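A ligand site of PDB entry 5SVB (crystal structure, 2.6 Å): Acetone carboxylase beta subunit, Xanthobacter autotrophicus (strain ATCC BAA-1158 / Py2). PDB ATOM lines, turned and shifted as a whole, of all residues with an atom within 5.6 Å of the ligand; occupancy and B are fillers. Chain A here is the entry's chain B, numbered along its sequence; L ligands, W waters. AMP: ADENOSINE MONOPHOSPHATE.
Residues that only touch the ligand: Ala 362 (3.1 Å), Phe 415 (3.2 Å), Thr 704 (3.3 Å), Gly 321 (3.4 Å), Leu 410 (3.5 Å), Ser 701 (3.6 Å), Ala 703 (3.6 Å), Gly 482 (3.7 Å) and Met 32 (3.8 Å).
Within 4 Å of the ligand: Thr 31, Met 32, Lys 48, Gly 321, Gly 322, Ala 362, Ser 401, Leu 410, Asn 414, Phe 415, Leu 416, Gly 482, Gly 483, Ala 484, Ser 701, Asp 702, Ala 703, Thr 704 and Thr 705.
Along chain A the residues within 4 Å of the ligand span positions 31 to 705.
The nearest printed residue that does not touch the ligand is Val 487 (4.2 Å).
N7 of the ligand sits at hydrogen-bond distance from OG1 of Thr 705 (3.2 Å).
O of Asp 702 sits at hydrogen-bond distance from N6 of the ligand (3.2 Å).
An oxygen (O2P) of the ligand lies within hydrogen-bond range of the side-chain hydroxyl (OG1) of Thr 31 (2.7 Å).
The backbone NH (N) of Gly 322 lies within hydrogen-bond range of an oxygen (O2P) of the ligand.
N of Leu 416 is in hydrogen-bond range of N1 of the ligand (2.9 Å).
O4' of the ligand is in hydrogen-bond range of N of Ala 484, 3.2 Å away.
The side-chain amino group (NZ) of Lys 48 is in salt-bridge range of an oxygen (O1P) of the ligand.
OG of Ser 401 is in hydrogen-bond range of O2' of the ligand (3.4 Å).
A nitrogen (N6) of the ligand sits at hydrogen-bond distance from the backbone carbonyl oxygen (O) of Asn 414 (3.0 Å).
N7 of the ligand sits at hydrogen-bond distance from N of Thr 705 (3.3 Å).
N of Gly 483 lies within hydrogen-bond range of O3P of the ligand, at 2.9 Å.
OG of Ser 701 sits at hydrogen-bond distance from OD1 of Asp 702.
The side-chain amide nitrogen of Asn 414 sits at hydrogen-bond distance from the backbone carbonyl oxygen of Ser 701.
The backbone carbonyl oxygen (O) of Asp 702 is in hydrogen-bond range of the backbone NH (N) of Gly 417, at 3.0 Å.
The side-chain amino group of Lys 48 is in salt-bridge range of the side-chain carboxylate of Asp 34, at 3.1 Å.
The backbone NH of Ala 484 sits at hydrogen-bond distance from the backbone carbonyl oxygen of Ile 320, at 2.9 Å.
O of Asp 702 lies close to N of Leu 416 (3.0 Å).
O of Ala 508 is in hydrogen-bond range of NZ of Lys 48 (2.6 Å).
O of Gly 483 is in hydrogen-bond range of OG1 of Thr 704 (3.0 Å).
Water W1 lies within hydrogen-bond range of O1P of the ligand (2.9 Å), O of Ala 703 (3.2 Å) and NZ of Lys 48 (3.4 Å).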
ATOM      1  N   GLY A  30      10.893  -0.100   6.891  1.00  0.00           N
ATOM      2  CA  GLY A  30      10.732  -1.194   7.823  1.00  0.00           C
ATOM      3  C   GLY A  30      10.784  -0.751   9.268  1.00  0.00           C
ATOM      4  O   GLY A  30      10.357   0.356   9.614  1.00  0.00           O
ATOM      5  N   THR A  31      11.311  -1.628  10.126  1.00  0.00           N
ATOM      6  CA  THR A  31      11.397  -1.325  11.545  1.00  0.00           C
ATOM      7  C   THR A  31      12.137  -0.020  11.782  1.00  0.00           C
ATOM      8  O   THR A  31      11.722   0.791  12.626  1.00  0.00           O
ATOM      9  CB  THR A  31      12.097  -2.465  12.282  1.00  0.00           C
ATOM     10  OG1 THR A  31      11.460  -3.707  11.962  1.00  0.00           O
ATOM     11  CG2 THR A  31      12.047  -2.249  13.786  1.00  0.00           C
ATOM     12  N   MET A  32      13.227   0.191  11.061  1.00  0.00           N
ATOM     13  CA  MET A  32      14.014   1.411  11.207  1.00  0.00           C
ATOM     14  C   MET A  32      14.700   1.720   9.874  1.00  0.00           C
ATOM     15  O   MET A  32      14.398   1.107   8.861  1.00  0.00           O
ATOM     16  CB  MET A  32      15.033   1.257  12.323  1.00  0.00           C
ATOM     17  CG  MET A  32      15.944   0.057  12.181  1.00  0.00           C
ATOM     18  SD  MET A  32      16.872  -0.361  13.843  1.00  0.00           S
ATOM     19  CE  MET A  32      16.661  -2.301  13.792  1.00  0.00           C
ATOM     20  N   ASP A  34      17.437   1.473   7.349  1.00  0.00           N
ATOM     21  CA  ASP A  34      18.550   0.631   6.946  1.00  0.00           C
ATOM     22  C   ASP A  34      19.357   1.325   5.858  1.00  0.00           C
ATOM     23  O   ASP A  34      18.801   1.964   4.963  1.00  0.00           O
ATOM     24  CB  ASP A  34      18.050  -0.718   6.418  1.00  0.00           C
ATOM     25  CG  ASP A  34      17.189  -1.448   7.420  1.00  0.00           C
ATOM     26  OD1 ASP A  34      17.172  -1.054   8.598  1.00  0.00           O
ATOM     27  OD2 ASP A  34      16.543  -2.445   7.021  1.00  0.00           O
ATOM     28  N   LYS A  48      22.177   0.765  10.794  1.00  0.00           N
ATOM     29  CA  LYS A  48      20.859   0.707  11.423  1.00  0.00           C
ATOM     30  C   LYS A  48      20.701   1.876  12.366  1.00  0.00           C
ATOM     31  O   LYS A  48      21.594   2.143  13.180  1.00  0.00           O
ATOM     32  CB  LYS A  48      20.667  -0.615  12.175  1.00  0.00           C
ATOM     33  CG  LYS A  48      20.699  -1.861  11.302  1.00  0.00           C
ATOM     34  CD  LYS A  48      19.334  -2.170  10.720  1.00  0.00           C
ATOM     35  CE  LYS A  48      19.303  -3.567  10.131  1.00  0.00           C
ATOM     36  NZ  LYS A  48      17.978  -3.887   9.528  1.00  0.00           N
ATOM     37  N   ASP A 319      11.377 -12.305   4.117  1.00  0.00           N
ATOM     38  CA  ASP A 319      11.895 -11.137   4.827  1.00  0.00           C
ATOM     39  C   ASP A 319      11.235 -11.104   6.205  1.00  0.00           C
ATOM     40  O   ASP A 319      10.104 -10.622   6.354  1.00  0.00           O
ATOM     41  CB  ASP A 319      11.602  -9.857   4.055  1.00  0.00           C
ATOM     42  CG  ASP A 319      12.317  -8.655   4.630  1.00  0.00           C
ATOM     43  OD1 ASP A 319      12.634  -8.656   5.843  1.00  0.00           O
ATOM     44  OD2 ASP A 319      12.576  -7.691   3.870  1.00  0.00           O
ATOM     45  N   ILE A 320      11.947 -11.606   7.209  1.00  0.00           N
ATOM     46  CA  ILE A 320      11.449 -11.646   8.580  1.00  0.00           C
ATOM     47  C   ILE A 320      12.071 -10.464   9.299  1.00  0.00           C
ATOM     48  O   ILE A 320      13.215 -10.516   9.748  1.00  0.00           O
ATOM     49  CB  ILE A 320      11.809 -12.971   9.272  1.00  0.00           C
ATOM     50  CG1 ILE A 320      11.419 -14.160   8.389  1.00  0.00           C
ATOM     51  CG2 ILE A 320      11.120 -13.062  10.621  1.00  0.00           C
ATOM     52  CD1 ILE A 320       9.948 -14.234   8.038  1.00  0.00           C
ATOM     53  N   GLY A 321      11.297  -9.381   9.429  1.00  0.00           N
ATOM     54  CA  GLY A 321      11.765  -8.171  10.077  1.00  0.00           C
ATOM     55  C   GLY A 321      11.169  -8.002  11.464  1.00  0.00           C
ATOM     56  O   GLY A 321      10.571  -8.910  12.050  1.00  0.00           O
ATOM     57  N   GLY A 322      11.361  -6.798  12.009  1.00  0.00           N
ATOM     58  CA  GLY A 322      10.792  -6.469  13.298  1.00  0.00           C
ATOM     59  C   GLY A 322       9.341  -6.047  13.250  1.00  0.00           C
ATOM     60  O   GLY A 322       8.655  -6.116  14.275  1.00  0.00           O
ATOM     61  N   THR A 323       8.855  -5.620  12.090  1.00  0.00           N
ATOM     62  CA  THR A 323       7.484  -5.143  11.954  1.00  0.00           C
ATOM     63  C   THR A 323       6.645  -5.932  10.963  1.00  0.00           C
ATOM     64  O   THR A 323       5.440  -5.696  10.891  1.00  0.00           O
ATOM     65  CB  THR A 323       7.471  -3.665  11.520  1.00  0.00           C
ATOM     66  OG1 THR A 323       8.214  -3.508  10.304  1.00  0.00           O
ATOM     67  CG2 THR A 323       8.063  -2.781  12.598  1.00  0.00           C
ATOM     68  N   ALA A 362       9.116  -9.716  14.173  1.00  0.00           N
ATOM     69  CA  ALA A 362       9.605 -10.287  15.421  1.00  0.00           C
ATOM     70  C   ALA A 362       9.114  -9.516  16.637  1.00  0.00           C
ATOM     71  O   ALA A 362       9.179 -10.021  17.755  1.00  0.00           O
ATOM     72  CB  ALA A 362      11.135 -10.340  15.417  1.00  0.00           C
ATOM     73  N   GLY A 363       8.636  -8.288  16.443  1.00  0.00           N
ATOM     74  CA  GLY A 363       8.026  -7.530  17.504  1.00  0.00           C
ATOM     75  C   GLY A 363       6.569  -7.828  17.725  1.00  0.00           C
ATOM     76  O   GLY A 363       5.904  -7.113  18.493  1.00  0.00           O
ATOM     77  N   GLY A 383       7.828  -3.410  17.352  1.00  0.00           N
ATOM     78  CA  GLY A 383       8.642  -2.710  16.381  1.00  0.00           C
ATOM     79  C   GLY A 383      10.014  -2.367  16.948  1.00  0.00           C
ATOM     80  O   GLY A 383      10.705  -3.229  17.502  1.00  0.00           O
ATOM     81  N   SER A 401      10.305 -11.453  20.065  1.00  0.00           N
ATOM     82  CA  SER A 401      11.689 -11.209  20.454  1.00  0.00           C
ATOM     83  C   SER A 401      11.936 -11.626  21.899  1.00  0.00           C
ATOM     84  O   SER A 401      13.026 -12.110  22.225  1.00  0.00           O
ATOM     85  CB  SER A 401      12.051  -9.741  20.249  1.00  0.00           C
ATOM     86  OG  SER A 401      12.262  -9.464  18.881  1.00  0.00           O
ATOM     87  N   HIS A 404      12.812 -15.128  21.916  1.00  0.00           N
ATOM     88  CA  HIS A 404      14.193 -15.332  21.514  1.00  0.00           C
ATOM     89  C   HIS A 404      15.158 -15.106  22.675  1.00  0.00           C
ATOM     90  O   HIS A 404      16.239 -15.705  22.705  1.00  0.00           O
ATOM     91  CB  HIS A 404      14.548 -14.408  20.357  1.00  0.00           C
ATOM     92  CG  HIS A 404      13.801 -14.688  19.102  1.00  0.00           C
ATOM     93  ND1 HIS A 404      13.696 -13.771  18.071  1.00  0.00           N
ATOM     94  CD2 HIS A 404      13.115 -15.785  18.693  1.00  0.00           C
ATOM     95  CE1 HIS A 404      12.986 -14.295  17.091  1.00  0.00           C
ATOM     96  NE2 HIS A 404      12.619 -15.512  17.442  1.00  0.00           N
ATOM     97  N   LEU A 410      18.947 -14.983  20.891  1.00  0.00           N
ATOM     98  CA  LEU A 410      19.525 -13.653  20.793  1.00  0.00           C
ATOM     99  C   LEU A 410      20.483 -13.386  21.948  1.00  0.00           C
ATOM    100  O   LEU A 410      20.311 -13.907  23.049  1.00  0.00           O
ATOM    101  CB  LEU A 410      18.431 -12.585  20.783  1.00  0.00           C
ATOM    102  CG  LEU A 410      17.540 -12.531  19.538  1.00  0.00           C
ATOM    103  CD1 LEU A 410      16.356 -11.626  19.814  1.00  0.00           C
ATOM    104  CD2 LEU A 410      18.308 -12.037  18.337  1.00  0.00           C
ATOM    105  N   ASN A 414      24.189  -7.857  22.663  1.00  0.00           N
ATOM    106  CA  ASN A 414      24.622  -7.591  21.299  1.00  0.00           C
ATOM    107  C   ASN A 414      23.459  -7.204  20.400  1.00  0.00           C
ATOM    108  O   ASN A 414      23.497  -7.435  19.191  1.00  0.00           O
ATOM    109  CB  ASN A 414      25.335  -8.814  20.714  1.00  0.00           C
ATOM    110  CG  ASN A 414      26.137  -8.476  19.476  1.00  0.00           C
ATOM    111  OD1 ASN A 414      26.485  -7.319  19.251  1.00  0.00           O
ATOM    112  ND2 ASN A 414      26.443  -9.484  18.679  1.00  0.00           N
ATOM    113  N   PHE A 415      22.412  -6.595  20.970  1.00  0.00           N
ATOM    114  CA  PHE A 415      21.286  -6.123  20.177  1.00  0.00           C
ATOM    115  C   PHE A 415      21.659  -4.768  19.580  1.00  0.00           C
ATOM    116  O   PHE A 415      21.788  -3.780  20.311  1.00  0.00           O
ATOM    117  CB  PHE A 415      20.034  -6.022  21.033  1.00  0.00           C
ATOM    118  CG  PHE A 415      18.763  -5.945  20.245  1.00  0.00           C
ATOM    119  CD1 PHE A 415      18.249  -4.716  19.851  1.00  0.00           C
ATOM    120  CD2 PHE A 415      18.082  -7.090  19.891  1.00  0.00           C
ATOM    121  CE1 PHE A 415      17.080  -4.641  19.115  1.00  0.00           C
ATOM    122  CE2 PHE A 415      16.908  -7.020  19.162  1.00  0.00           C
ATOM    123  CZ  PHE A 415      16.412  -5.797  18.776  1.00  0.00           C
ATOM    124  N   LEU A 416      21.839  -4.725  18.259  1.00  0.00           N
ATOM    125  CA  LEU A 416      22.349  -3.541  17.588  1.00  0.00           C
ATOM    126  C   LEU A 416      23.736  -3.184  18.133  1.00  0.00           C
ATOM    127  O   LEU A 416      24.023  -2.038  18.472  1.00  0.00           O
ATOM    128  CB  LEU A 416      21.384  -2.360  17.708  1.00  0.00           C
ATOM    129  CG  LEU A 416      20.008  -2.552  17.059  1.00  0.00           C
ATOM    130  CD1 LEU A 416      19.170  -1.292  17.233  1.00  0.00           C
ATOM    131  CD2 LEU A 416      20.113  -2.908  15.583  1.00  0.00           C
ATOM    132  N   GLY A 417      24.579  -4.202  18.227  1.00  0.00           N
ATOM    133  CA  GLY A 417      25.897  -4.044  18.803  1.00  0.00           C
ATOM    134  C   GLY A 417      25.912  -3.787  20.295  1.00  0.00           C
ATOM    135  O   GLY A 417      26.979  -3.548  20.853  1.00  0.00           O
ATOM    136  N   GLY A 482      16.388 -10.176   6.298  1.00  0.00           N
ATOM    137  CA  GLY A 482      15.836  -9.414   7.387  1.00  0.00           C
ATOM    138  C   GLY A 482      16.558  -9.701   8.684  1.00  0.00           C
ATOM    139  O   GLY A 482      17.230 -10.717   8.856  1.00  0.00           O
ATOM    140  N   GLY A 483      16.419  -8.777   9.632  1.00  0.00           N
ATOM    141  CA  GLY A 483      17.109  -8.925  10.902  1.00  0.00           C
ATOM    142  C   GLY A 483      16.789 -10.236  11.590  1.00  0.00           C
ATOM    143  O   GLY A 483      17.648 -10.811  12.263  1.00  0.00           O
ATOM    144  N   ALA A 484      15.567 -10.732  11.445  1.00  0.00           N
ATOM    145  CA  ALA A 484      15.111 -11.909  12.156  1.00  0.00           C
ATOM    146  C   ALA A 484      14.942 -13.133  11.261  1.00  0.00           C
ATOM    147  O   ALA A 484      14.549 -14.196  11.760  1.00  0.00           O
ATOM    148  CB  ALA A 484      13.786 -11.608  12.861  1.00  0.00           C
ATOM    149  N   VAL A 487      17.103 -16.044  12.123  1.00  0.00           N
ATOM    150  CA  VAL A 487      16.759 -16.615  13.418  1.00  0.00           C
ATOM    151  C   VAL A 487      15.769 -17.764  13.266  1.00  0.00           C
ATOM    152  O   VAL A 487      15.714 -18.650  14.115  1.00  0.00           O
ATOM    153  CB  VAL A 487      16.194 -15.527  14.341  1.00  0.00           C
ATOM    154  CG1 VAL A 487      16.015 -16.071  15.749  1.00  0.00           C
ATOM    155  CG2 VAL A 487      17.100 -14.304  14.350  1.00  0.00           C
ATOM    156  N   ALA A 508      20.601  -8.367   7.232  1.00  0.00           N
ATOM    157  CA  ALA A 508      19.993  -7.245   7.944  1.00  0.00           C
ATOM    158  C   ALA A 508      19.774  -6.033   7.055  1.00  0.00           C
ATOM    159  O   ALA A 508      19.064  -5.112   7.462  1.00  0.00           O
ATOM    160  CB  ALA A 508      20.863  -6.854   9.135  1.00  0.00           C
ATOM    161  N   SER A 701      25.845 -11.428  14.336  1.00  0.00           N
ATOM    162  CA  SER A 701      26.259 -10.141  13.804  1.00  0.00           C
ATOM    163  C   SER A 701      25.760  -9.059  14.752  1.00  0.00           C
ATOM    164  O   SER A 701      25.158  -9.343  15.790  1.00  0.00           O
ATOM    165  CB  SER A 701      25.722  -9.944  12.381  1.00  0.00           C
ATOM    166  OG  SER A 701      26.064  -8.654  11.884  1.00  0.00           O
ATOM    167  N   ASP A 702      26.004  -7.801  14.401  1.00  0.00           N
ATOM    168  CA  ASP A 702      25.562  -6.709  15.258  1.00  0.00           C
ATOM    169  C   ASP A 702      24.090  -6.382  15.081  1.00  0.00           C
ATOM    170  O   ASP A 702      23.487  -5.810  15.988  1.00  0.00           O
ATOM    171  CB  ASP A 702      26.412  -5.455  15.005  1.00  0.00           C
ATOM    172  CG  ASP A 702      26.211  -4.879  13.626  1.00  0.00           C
ATOM    173  OD1 ASP A 702      25.656  -5.588  12.752  1.00  0.00           O
ATOM    174  OD2 ASP A 702      26.617  -3.722  13.399  1.00  0.00           O
ATOM    175  N   ALA A 703      23.489  -6.757  13.943  1.00  0.00           N
ATOM    176  CA  ALA A 703      22.088  -6.471  13.678  1.00  0.00           C
ATOM    177  C   ALA A 703      21.346  -7.675  13.110  1.00  0.00           C
ATOM    178  O   ALA A 703      20.277  -7.520  12.519  1.00  0.00           O
ATOM    179  CB  ALA A 703      21.955  -5.281  12.709  1.00  0.00           C
ATOM    180  N   THR A 704      21.888  -8.878  13.281  1.00  0.00           N
ATOM    181  CA  THR A 704      21.186 -10.096  12.893  1.00  0.00           C
ATOM    182  C   THR A 704      21.872 -11.288  13.546  1.00  0.00           C
ATOM    183  O   THR A 704      23.069 -11.248  13.818  1.00  0.00           O
ATOM    184  CB  THR A 704      21.140 -10.276  11.376  1.00  0.00           C
ATOM    185  OG1 THR A 704      20.350 -11.435  11.050  1.00  0.00           O
ATOM    186  CG2 THR A 704      22.526 -10.451  10.805  1.00  0.00           C
ATOM    187  N   THR A 705      21.081 -12.336  13.793  1.00  0.00           N
ATOM    188  CA  THR A 705      21.578 -13.558  14.411  1.00  0.00           C
ATOM    189  C   THR A 705      21.128 -14.746  13.584  1.00  0.00           C
ATOM    190  O   THR A 705      19.952 -14.858  13.239  1.00  0.00           O
ATOM    191  CB  THR A 705      21.074 -13.693  15.853  1.00  0.00           C
ATOM    192  OG1 THR A 705      21.339 -12.485  16.570  1.00  0.00           O
ATOM    193  CG2 THR A 705      21.756 -14.847  16.541  1.00  0.00           C
HETATM  194  P   AMP L   1      14.712  -5.688  10.608  1.00  0.00           P
HETATM  195  O1P AMP L   1      15.819  -4.708  10.934  1.00  0.00           O
HETATM  196  O2P AMP L   1      13.303  -5.187  10.599  1.00  0.00           O
HETATM  197  O3P AMP L   1      15.013  -6.289   9.254  1.00  0.00           O
HETATM  198  O5' AMP L   1      14.795  -6.842  11.690  1.00  0.00           O
HETATM  199  C5' AMP L   1      14.729  -6.560  13.076  1.00  0.00           C
HETATM  200  C4' AMP L   1      14.664  -7.823  13.895  1.00  0.00           C
HETATM  201  O4' AMP L   1      15.903  -8.538  13.765  1.00  0.00           O
HETATM  202  C3' AMP L   1      14.515  -7.629  15.402  1.00  0.00           C
HETATM  203  O3' AMP L   1      13.170  -7.413  15.782  1.00  0.00           O
HETATM  204  C2' AMP L   1      15.108  -8.916  15.986  1.00  0.00           C
HETATM  205  O2' AMP L   1      14.124  -9.926  16.131  1.00  0.00           O
HETATM  206  C1' AMP L   1      16.111  -9.341  14.908  1.00  0.00           C
HETATM  207  N9  AMP L   1      17.487  -9.139  15.360  1.00  0.00           N
HETATM  208  C8  AMP L   1      18.131 -10.298  15.206  1.00  0.00           C
HETATM  209  N7  AMP L   1      19.386 -10.120  15.630  1.00  0.00           N
HETATM  210  C5  AMP L   1      19.503  -8.845  16.036  1.00  0.00           C
HETATM  211  C6  AMP L   1      20.532  -8.121  16.553  1.00  0.00           C
HETATM  212  N6  AMP L   1      21.909  -8.406  16.871  1.00  0.00           N
HETATM  213  N1  AMP L   1      20.356  -6.848  16.872  1.00  0.00           N
HETATM  214  C2  AMP L   1      19.161  -6.261  16.705  1.00  0.00           C
HETATM  215  N3  AMP L   1      18.137  -6.964  16.191  1.00  0.00           N
HETATM  216  C4  AMP L   1      18.322  -8.256  15.866  1.00  0.00           C
HETATM  217  O   HOH W   1      18.177  -5.170  12.640  1.00  0.00           O
